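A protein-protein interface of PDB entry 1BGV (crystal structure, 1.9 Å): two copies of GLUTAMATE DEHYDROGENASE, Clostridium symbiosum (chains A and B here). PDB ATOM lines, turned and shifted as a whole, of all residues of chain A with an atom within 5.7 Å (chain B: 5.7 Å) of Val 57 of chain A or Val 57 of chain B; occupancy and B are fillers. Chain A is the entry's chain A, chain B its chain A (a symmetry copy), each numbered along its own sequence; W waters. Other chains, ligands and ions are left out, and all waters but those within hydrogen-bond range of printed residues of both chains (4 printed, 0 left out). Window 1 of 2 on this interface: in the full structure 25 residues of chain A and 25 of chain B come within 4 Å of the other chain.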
ATOM      1  N   PRO A  54      -0.868  10.621 -20.761  1.00  0.00           N
ATOM      2  CA  PRO A  54      -1.879   9.562 -20.711  1.00  0.00           C
ATOM      3  C   PRO A  54      -1.210   8.246 -20.267  1.00  0.00           C
ATOM      4  O   PRO A  54      -0.022   7.957 -20.617  1.00  0.00           O
ATOM      5  CB  PRO A  54      -2.368   9.408 -22.166  1.00  0.00           C
ATOM      6  CG  PRO A  54      -1.788  10.503 -22.931  1.00  0.00           C
ATOM      7  CD  PRO A  54      -0.756  11.254 -22.081  1.00  0.00           C
ATOM      8  N   GLU A  55      -1.981   7.398 -19.568  1.00  0.00           N
ATOM      9  CA  GLU A  55      -1.393   6.098 -19.229  1.00  0.00           C
ATOM     10  C   GLU A  55      -0.938   5.397 -20.469  1.00  0.00           C
ATOM     11  O   GLU A  55       0.148   4.821 -20.502  1.00  0.00           O
ATOM     12  CB  GLU A  55      -2.372   5.230 -18.390  1.00  0.00           C
ATOM     13  CG  GLU A  55      -2.585   5.873 -17.014  1.00  0.00           C
ATOM     14  CD  GLU A  55      -3.670   5.248 -16.220  1.00  0.00           C
ATOM     15  OE1 GLU A  55      -3.999   4.067 -16.444  1.00  0.00           O
ATOM     16  OE2 GLU A  55      -4.055   5.826 -15.170  1.00  0.00           O
ATOM     17  N   ARG A  56      -1.811   5.350 -21.482  1.00  0.00           N
ATOM     18  CA  ARG A  56      -1.517   4.543 -22.655  1.00  0.00           C
ATOM     19  C   ARG A  56      -2.188   5.239 -23.847  1.00  0.00           C
ATOM     20  O   ARG A  56      -3.334   5.687 -23.729  1.00  0.00           O
ATOM     21  CB  ARG A  56      -2.175   3.161 -22.422  1.00  0.00           C
ATOM     22  CG  ARG A  56      -1.716   2.158 -23.367  1.00  0.00           C
ATOM     23  CD  ARG A  56      -2.498   0.828 -23.151  1.00  0.00           C
ATOM     24  NE  ARG A  56      -2.071   0.158 -21.919  1.00  0.00           N
ATOM     25  CZ  ARG A  56      -2.770   0.163 -20.789  1.00  0.00           C
ATOM     26  NH1 ARG A  56      -3.986   0.763 -20.709  1.00  0.00           N
ATOM     27  NH2 ARG A  56      -2.233  -0.380 -19.665  1.00  0.00           N
ATOM     28  N   VAL A  57      -1.482   5.266 -24.978  1.00  0.00           N
ATOM     29  CA  VAL A  57      -2.048   5.782 -26.224  1.00  0.00           C
ATOM     30  C   VAL A  57      -1.882   4.670 -27.253  1.00  0.00           C
ATOM     31  O   VAL A  57      -0.800   4.068 -27.384  1.00  0.00           O
ATOM     32  CB  VAL A  57      -1.255   7.019 -26.756  1.00  0.00           C
ATOM     33  CG1 VAL A  57      -1.637   7.351 -28.202  1.00  0.00           C
ATOM     34  CG2 VAL A  57      -1.479   8.187 -25.874  1.00  0.00           C
ATOM     35  N   ILE A  58      -2.925   4.412 -28.041  1.00  0.00           N
ATOM     36  CA  ILE A  58      -2.806   3.412 -29.102  1.00  0.00           C
ATOM     37  C   ILE A  58      -3.235   4.113 -30.399  1.00  0.00           C
ATOM     38  O   ILE A  58      -4.316   4.734 -30.433  1.00  0.00           O
ATOM     39  CB  ILE A  58      -3.803   2.193 -28.871  1.00  0.00           C
ATOM     40  CG1 ILE A  58      -3.482   1.420 -27.565  1.00  0.00           C
ATOM     41  CG2 ILE A  58      -3.728   1.204 -30.064  1.00  0.00           C
ATOM     42  CD1 ILE A  58      -4.687   1.432 -26.667  1.00  0.00           C
ATOM     43  N   GLU A  59      -2.428   3.973 -31.449  1.00  0.00           N
ATOM     44  CA  GLU A  59      -2.864   4.453 -32.781  1.00  0.00           C
ATOM     45  C   GLU A  59      -2.758   3.249 -33.689  1.00  0.00           C
ATOM     46  O   GLU A  59      -1.767   2.507 -33.584  1.00  0.00           O
ATOM     47  CB  GLU A  59      -1.880   5.466 -33.420  1.00  0.00           C
ATOM     48  CG  GLU A  59      -1.890   6.749 -32.711  1.00  0.00           C
ATOM     49  CD  GLU A  59      -1.004   7.854 -33.360  1.00  0.00           C
ATOM     50  OE1 GLU A  59      -0.766   7.769 -34.651  1.00  0.00           O
ATOM     51  OE2 GLU A  59      -0.777   8.861 -32.723  1.00  0.00           O
ATOM     52  N   PHE A  60      -3.640   3.126 -34.683  1.00  0.00           N
ATOM     53  CA  PHE A  60      -3.488   1.982 -35.570  1.00  0.00           C
ATOM     54  C   PHE A  60      -4.013   2.265 -36.973  1.00  0.00           C
ATOM     55  O   PHE A  60      -4.915   3.098 -37.166  1.00  0.00           O
ATOM     56  CB  PHE A  60      -4.218   0.721 -34.979  1.00  0.00           C
ATOM     57  CG  PHE A  60      -5.621   1.014 -34.465  1.00  0.00           C
ATOM     58  CD1 PHE A  60      -5.814   1.627 -33.223  1.00  0.00           C
ATOM     59  CD2 PHE A  60      -6.772   0.729 -35.243  1.00  0.00           C
ATOM     60  CE1 PHE A  60      -7.097   1.893 -32.712  1.00  0.00           C
ATOM     61  CE2 PHE A  60      -8.053   0.986 -34.727  1.00  0.00           C
ATOM     62  CZ  PHE A  60      -8.203   1.595 -33.468  1.00  0.00           C
ATOM     63  N   ARG A  78      -6.950   5.532 -29.703  1.00  0.00           N
ATOM     64  CA  ARG A  78      -7.681   5.423 -28.436  1.00  0.00           C
ATOM     65  C   ARG A  78      -6.641   5.922 -27.408  1.00  0.00           C
ATOM     66  O   ARG A  78      -5.564   5.339 -27.282  1.00  0.00           O
ATOM     67  CB  ARG A  78      -8.133   3.959 -28.125  1.00  0.00           C
ATOM     68  CG  ARG A  78      -8.952   3.879 -26.842  1.00  0.00           C
ATOM     69  CD  ARG A  78     -10.265   4.615 -26.950  1.00  0.00           C
ATOM     70  NE  ARG A  78     -11.142   4.381 -25.800  1.00  0.00           N
ATOM     71  CZ  ARG A  78     -12.270   5.065 -25.588  1.00  0.00           C
ATOM     72  NH1 ARG A  78     -12.663   6.018 -26.475  1.00  0.00           N
ATOM     73  NH2 ARG A  78     -13.014   4.830 -24.493  1.00  0.00           N
ATOM     74  N   VAL A  79      -6.981   6.970 -26.682  1.00  0.00           N
ATOM     75  CA  VAL A  79      -6.092   7.495 -25.697  1.00  0.00           C
ATOM     76  C   VAL A  79      -6.708   7.094 -24.365  1.00  0.00           C
ATOM     77  O   VAL A  79      -7.844   7.502 -24.058  1.00  0.00           O
ATOM     78  CB  VAL A  79      -6.071   9.061 -25.834  1.00  0.00           C
ATOM     79  CG1 VAL A  79      -5.302   9.669 -24.616  1.00  0.00           C
ATOM     80  CG2 VAL A  79      -5.338   9.459 -27.175  1.00  0.00           C
ATOM     81  N   GLN A  80      -6.018   6.218 -23.632  1.00  0.00           N
ATOM     82  CA  GLN A  80      -6.492   5.755 -22.297  1.00  0.00           C
ATOM     83  C   GLN A  80      -5.742   6.624 -21.255  1.00  0.00           C
ATOM     84  O   GLN A  80      -4.611   6.385 -20.844  1.00  0.00           O
ATOM     85  CB  GLN A  80      -6.254   4.224 -22.092  1.00  0.00           C
ATOM     86  CG  GLN A  80      -7.046   3.433 -23.152  1.00  0.00           C
ATOM     87  CD  GLN A  80      -6.750   1.948 -23.197  1.00  0.00           C
ATOM     88  OE1 GLN A  80      -5.672   1.506 -22.816  1.00  0.00           O
ATOM     89  NE2 GLN A  80      -7.719   1.148 -23.735  1.00  0.00           N
ATOM     90  N   LEU A 100      -3.979  13.242 -32.868  1.00  0.00           N
ATOM     91  CA  LEU A 100      -3.639  12.955 -31.462  1.00  0.00           C
ATOM     92  C   LEU A 100      -3.941  14.150 -30.525  1.00  0.00           C
ATOM     93  O   LEU A 100      -4.455  13.985 -29.406  1.00  0.00           O
ATOM     94  CB  LEU A 100      -2.165  12.475 -31.348  1.00  0.00           C
ATOM     95  CG  LEU A 100      -1.816  12.028 -29.918  1.00  0.00           C
ATOM     96  CD1 LEU A 100      -2.734  10.815 -29.414  1.00  0.00           C
ATOM     97  CD2 LEU A 100      -0.314  11.633 -29.931  1.00  0.00           C
ATOM     98  N   LYS A 104      -6.127  13.822 -27.176  1.00  0.00           N
ATOM     99  CA  LYS A 104      -5.636  14.028 -25.827  1.00  0.00           C
ATOM    100  C   LYS A 104      -6.399  15.127 -25.151  1.00  0.00           C
ATOM    101  O   LYS A 104      -6.722  15.037 -23.991  1.00  0.00           O
ATOM    102  CB  LYS A 104      -4.155  14.386 -25.859  1.00  0.00           C
ATOM    103  CG  LYS A 104      -3.299  13.228 -26.326  1.00  0.00           C
ATOM    104  CD  LYS A 104      -1.766  13.558 -26.382  1.00  0.00           C
ATOM    105  CE  LYS A 104      -1.284  14.297 -25.130  1.00  0.00           C
ATOM    106  NZ  LYS A 104       0.175  14.569 -25.343  1.00  0.00           N
ATOM    107  N   PRO B  54       1.985   2.951 -39.652  1.00  0.00           N
ATOM    108  CA  PRO B  54       2.391   1.771 -38.884  1.00  0.00           C
ATOM    109  C   PRO B  54       1.142   0.936 -38.541  1.00  0.00           C
ATOM    110  O   PRO B  54       0.025   1.491 -38.289  1.00  0.00           O
ATOM    111  CB  PRO B  54       2.990   2.333 -37.577  1.00  0.00           C
ATOM    112  CG  PRO B  54       3.096   3.775 -37.739  1.00  0.00           C
ATOM    113  CD  PRO B  54       2.386   4.217 -39.024  1.00  0.00           C
ATOM    114  N   GLU B  55       1.324  -0.390 -38.447  1.00  0.00           N
ATOM    115  CA  GLU B  55       0.170  -1.187 -38.020  1.00  0.00           C
ATOM    116  C   GLU B  55      -0.341  -0.694 -36.704  1.00  0.00           C
ATOM    117  O   GLU B  55      -1.549  -0.566 -36.506  1.00  0.00           O
ATOM    118  CB  GLU B  55       0.504  -2.705 -37.988  1.00  0.00           C
ATOM    119  CG  GLU B  55       0.755  -3.210 -39.413  1.00  0.00           C
ATOM    120  CD  GLU B  55       1.298  -4.588 -39.476  1.00  0.00           C
ATOM    121  OE1 GLU B  55       1.095  -5.377 -38.532  1.00  0.00           O
ATOM    122  OE2 GLU B  55       1.724  -5.017 -40.581  1.00  0.00           O
ATOM    123  N   ARG B  56       0.571  -0.502 -35.743  1.00  0.00           N
ATOM    124  CA  ARG B  56       0.143  -0.192 -34.390  1.00  0.00           C
ATOM    125  C   ARG B  56       1.239   0.688 -33.773  1.00  0.00           C
ATOM    126  O   ARG B  56       2.428   0.398 -33.948  1.00  0.00           O
ATOM    127  CB  ARG B  56       0.064  -1.536 -33.626  1.00  0.00           C
ATOM    128  CG  ARG B  56      -0.634  -1.418 -32.357  1.00  0.00           C
ATOM    129  CD  ARG B  56      -0.578  -2.775 -31.593  1.00  0.00           C
ATOM    130  NE  ARG B  56      -1.454  -3.769 -32.217  1.00  0.00           N
ATOM    131  CZ  ARG B  56      -1.023  -4.764 -32.986  1.00  0.00           C
ATOM    132  NH1 ARG B  56       0.301  -4.963 -33.213  1.00  0.00           N
ATOM    133  NH2 ARG B  56      -1.922  -5.560 -33.620  1.00  0.00           N
ATOM    134  N   VAL B  57       0.816   1.707 -33.024  1.00  0.00           N
ATOM    135  CA  VAL B  57       1.748   2.547 -32.273  1.00  0.00           C
ATOM    136  C   VAL B  57       1.273   2.513 -30.824  1.00  0.00           C
ATOM    137  O   VAL B  57       0.074   2.681 -30.536  1.00  0.00           O
ATOM    138  CB  VAL B  57       1.693   4.038 -32.738  1.00  0.00           C
ATOM    139  CG1 VAL B  57       2.414   4.961 -31.749  1.00  0.00           C
ATOM    140  CG2 VAL B  57       2.269   4.172 -34.095  1.00  0.00           C
ATOM    141  N   ILE B  58       2.202   2.352 -29.885  1.00  0.00           N
ATOM    142  CA  ILE B  58       1.824   2.391 -28.472  1.00  0.00           C
ATOM    143  C   ILE B  58       2.727   3.445 -27.816  1.00  0.00           C
ATOM    144  O   ILE B  58       3.962   3.390 -27.989  1.00  0.00           O
ATOM    145  CB  ILE B  58       2.117   1.003 -27.751  1.00  0.00           C
ATOM    146  CG1 ILE B  58       1.274  -0.153 -28.353  1.00  0.00           C
ATOM    147  CG2 ILE B  58       1.803   1.109 -26.236  1.00  0.00           C
ATOM    148  CD1 ILE B  58       2.192  -1.228 -28.863  1.00  0.00           C
ATOM    149  N   GLU B  59       2.127   4.351 -27.046  1.00  0.00           N
ATOM    150  CA  GLU B  59       2.943   5.278 -26.228  1.00  0.00           C
ATOM    151  C   GLU B  59       2.459   5.082 -24.809  1.00  0.00           C
ATOM    152  O   GLU B  59       1.239   4.976 -24.603  1.00  0.00           O
ATOM    153  CB  GLU B  59       2.637   6.771 -26.504  1.00  0.00           C
ATOM    154  CG  GLU B  59       3.104   7.182 -27.832  1.00  0.00           C
ATOM    155  CD  GLU B  59       2.926   8.698 -28.140  1.00  0.00           C
ATOM    156  OE1 GLU B  59       2.890   9.531 -27.122  1.00  0.00           O
ATOM    157  OE2 GLU B  59       3.074   9.077 -29.283  1.00  0.00           O
ATOM    158  N   PHE B  60       3.342   5.209 -23.815  1.00  0.00           N
ATOM    159  CA  PHE B  60       2.841   5.061 -22.458  1.00  0.00           C
ATOM    160  C   PHE B  60       3.659   5.861 -21.450  1.00  0.00           C
ATOM    161  O   PHE B  60       4.856   6.123 -21.657  1.00  0.00           O
ATOM    162  CB  PHE B  60       2.822   3.547 -22.034  1.00  0.00           C
ATOM    163  CG  PHE B  60       4.102   2.799 -22.382  1.00  0.00           C
ATOM    164  CD1 PHE B  60       4.342   2.364 -23.690  1.00  0.00           C
ATOM    165  CD2 PHE B  60       5.113   2.568 -21.416  1.00  0.00           C
ATOM    166  CE1 PHE B  60       5.505   1.655 -24.040  1.00  0.00           C
ATOM    167  CE2 PHE B  60       6.270   1.851 -21.764  1.00  0.00           C
ATOM    168  CZ  PHE B  60       6.468   1.422 -23.089  1.00  0.00           C
ATOM    169  N   ARG B  78       6.514   2.294 -28.611  1.00  0.00           N
ATOM    170  CA  ARG B  78       6.901   1.127 -29.411  1.00  0.00           C
ATOM    171  C   ARG B  78       6.042   1.298 -30.684  1.00  0.00           C
ATOM    172  O   ARG B  78       4.814   1.321 -30.606  1.00  0.00           O
ATOM    173  CB  ARG B  78       6.592  -0.226 -28.693  1.00  0.00           C
ATOM    174  CG  ARG B  78       7.066  -1.423 -29.510  1.00  0.00           C
ATOM    175  CD  ARG B  78       8.567  -1.461 -29.657  1.00  0.00           C
ATOM    176  NE  ARG B  78       9.045  -2.704 -30.268  1.00  0.00           N
ATOM    177  CZ  ARG B  78      10.309  -2.888 -30.661  1.00  0.00           C
ATOM    178  NH1 ARG B  78      11.226  -1.900 -30.484  1.00  0.00           N
ATOM    179  NH2 ARG B  78      10.677  -4.039 -31.252  1.00  0.00           N
ATOM    180  N   VAL B  79       6.692   1.396 -31.828  1.00  0.00           N
ATOM    181  CA  VAL B  79       5.984   1.543 -33.059  1.00  0.00           C
ATOM    182  C   VAL B  79       6.128   0.197 -33.753  1.00  0.00           C
ATOM    183  O   VAL B  79       7.259  -0.229 -34.053  1.00  0.00           O
ATOM    184  CB  VAL B  79       6.689   2.667 -33.904  1.00  0.00           C
ATOM    185  CG1 VAL B  79       6.087   2.674 -35.346  1.00  0.00           C
ATOM    186  CG2 VAL B  79       6.443   4.068 -33.219  1.00  0.00           C
ATOM    187  N   GLN B  80       5.009  -0.514 -33.907  1.00  0.00           N
ATOM    188  CA  GLN B  80       5.001  -1.838 -34.588  1.00  0.00           C
ATOM    189  C   GLN B  80       4.559  -1.563 -36.049  1.00  0.00           C
ATOM    190  O   GLN B  80       3.391  -1.462 -36.409  1.00  0.00           O
ATOM    191  CB  GLN B  80       4.072  -2.864 -33.860  1.00  0.00           C
ATOM    192  CG  GLN B  80       4.587  -3.097 -32.426  1.00  0.00           C
ATOM    193  CD  GLN B  80       3.669  -3.914 -31.540  1.00  0.00           C
ATOM    194  OE1 GLN B  80       2.461  -3.952 -31.746  1.00  0.00           O
ATOM    195  NE2 GLN B  80       4.251  -4.549 -30.477  1.00  0.00           N
ATOM    196  N   LEU B 100       7.875  10.613 -31.299  1.00  0.00           N
ATOM    197  CA  LEU B 100       7.217   9.725 -32.276  1.00  0.00           C
ATOM    198  C   LEU B 100       7.864   9.808 -33.680  1.00  0.00           C
ATOM    199  O   LEU B 100       8.059   8.791 -34.368  1.00  0.00           O
ATOM    200  CB  LEU B 100       5.687  10.000 -32.315  1.00  0.00           C
ATOM    201  CG  LEU B 100       4.946   8.996 -33.216  1.00  0.00           C
ATOM    202  CD1 LEU B 100       5.128   7.482 -32.723  1.00  0.00           C
ATOM    203  CD2 LEU B 100       3.452   9.417 -33.212  1.00  0.00           C
ATOM    204  N   LYS B 104       9.091   6.586 -35.732  1.00  0.00           N
ATOM    205  CA  LYS B 104       8.531   6.124 -36.988  1.00  0.00           C
ATOM    206  C   LYS B 104       9.583   6.096 -38.055  1.00  0.00           C
ATOM    207  O   LYS B 104       9.637   5.190 -38.851  1.00  0.00           O
ATOM    208  CB  LYS B 104       7.395   7.042 -37.422  1.00  0.00           C
ATOM    209  CG  LYS B 104       6.200   6.947 -36.497  1.00  0.00           C
ATOM    210  CD  LYS B 104       5.009   7.884 -36.904  1.00  0.00           C
ATOM    211  CE  LYS B 104       4.712   7.828 -38.406  1.00  0.00           C
ATOM    212  NZ  LYS B 104       3.585   8.789 -38.643  1.00  0.00           N
HETATM  213  O   HOH W   1       1.666   7.901 -36.789  1.00  0.00           O
HETATM  214  O   HOH W   2      -0.908   3.701 -36.638  1.00  0.00           O
HETATM  215  O   HOH W   3       1.518   7.995 -23.088  1.00  0.00           O
HETATM  216  O   HOH W   4       1.161  12.001 -25.935  1.00  0.00           O
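The backbone NH of Val 57 of chain A lies within hydrogen-bond range of the backbone carbonyl oxygen of Glu 59 of chain B (2.8 Å).
The backbone carbonyl oxygen (O) of Glu 59 of chain A lies within hydrogen-bond range of the backbone NH (N) of Val 57 of chain B, at 2.8 Å.
Glu 55 of chain A touches Phe 60 of chain B.
Glu 59 of chain B touches Arg 56 of chain A (O to CA, 3.4 Å).
Val 57 of chain A touches Val 57 of chain B (O to O, 3.6 Å).
Ile 58 of chain B touches Val 57 of chain A (CA to O, 3.3 Å).
Ile 58 of chain A touches Val 57 of chain B.
Arg 56 of chain B touches Glu 59 of chain A.
Phe 60 of chain A touches Glu 55 of chain B (CB to O, 3.3 Å).
Of the printed residues of chain B, Glu 55 of chain A touches Phe 60.
Printed residues of chain B within 4 Å of Ile 58 of chain A: Val 57 (3.3 Å).
Of the printed residues of chain B, Glu 59 of chain A touches Arg 56 and Val 57.
Arg 78 of chain A touches none of the printed residues of chain B.
Pro 54 of chain B touches none of the printed residues of chain A.
Val 57 of chain B touches just these residues of chain A: Val 57 (3.6 Å), Ile 58 (3.3 Å) and Glu 59 (2.8 Å).
Of the printed residues of chain A, Glu 59 of chain B touches Arg 56 (3.4 Å) and Val 57 (2.8 Å).
Glu 55 of chain A touches Phe 60 of chain B, and with the chains exchanged Phe 60 of chain A touches Glu 55 of chain B.
Arg 56 of chain A touches Glu 59 of chain B, and with the chains exchanged Glu 59 of chain A touches Arg 56 of chain B.
Val 57 of chain A touches Ile 58 of chain B, and with the chains exchanged Ile 58 of chain A touches Val 57 of chain B.
Val 57 of chain A touches Glu 59 of chain B, and with the chains exchanged Glu 59 of chain A touches Val 57 of chain B.
12 positions are printed for both chains.
Of the 9 pairs that touch across the chains among the printed residues, 9 have their exchanged pair printed and touching as well.
Of the 12 printed residues of chain B, 6 touch a printed residue of chain A.
Printed residues of chain B that touch a printed residue of chain A: Glu 55, Arg 56, Val 57, Ile 58, Glu 59 and Phe 60.
Hydrophobic or aromatic side chains of chain B that line the printed part of chain A: Val 57 and Phe 60.
Of the 12 printed residues of chain A, 6 touch a printed residue of chain B.
Printed residues of chain A that touch a printed residue of chain B: Glu 55, Arg 56, Val 57, Ile 58, Glu 59 and Phe 60.
Hydrophobic or aromatic side chains of chain A within 4 Å of the printed part of chain B: Val 57 and Phe 60.
N of Glu 55 of chain A lies within hydrogen-bond range of O of Gln 80 of chain A (3.1 Å).
The backbone carbonyl oxygen (O) of Arg 56 of chain A lies within hydrogen-bond range of the backbone NH (N) of Gln 80 of chain A (2.7 Å).
The backbone NH (N) of Arg 78 of chain A sits at hydrogen-bond distance from the backbone carbonyl oxygen (O) of Ile 58 of chain A (2.8 Å).
The backbone carbonyl oxygen (O) of Gln 80 of chain B sits at hydrogen-bond distance from the backbone NH (N) of Glu 55 of chain B, at 3.1 Å.
The backbone NH (N) of Gln 80 of chain B is in hydrogen-bond range of the backbone carbonyl oxygen (O) of Arg 56 of chain B, 2.7 Å away.
O of Ile 58 of chain B sits at hydrogen-bond distance from N of Arg 78 of chain B (2.8 Å).
Water W4 lies within hydrogen-bond range of the side-chain amino group of Lys 104 of chain A (2.8 Å) and the side-chain carboxylate of Glu 59 of chain B (3.2 Å).
Water W1 lies within hydrogen-bond range of NZ of Lys 104 of chain B (2.8 Å) and OE1 of Glu 59 of chain A (3.2 Å).
Water W3 lies within hydrogen-bond range of O of Pro 54 of chain A (2.9 Å), O of Glu 59 of chain B (3.4 Å) and N of Phe 60 of chain B (3.4 Å).
Water W2 lies within hydrogen-bond range of the backbone carbonyl oxygen (O) of Pro 54 of chain B (2.9 Å), the backbone carbonyl oxygen (O) of Glu 59 of chain A (3.4 Å) and the backbone NH (N) of Phe 60 of chain A (3.4 Å).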
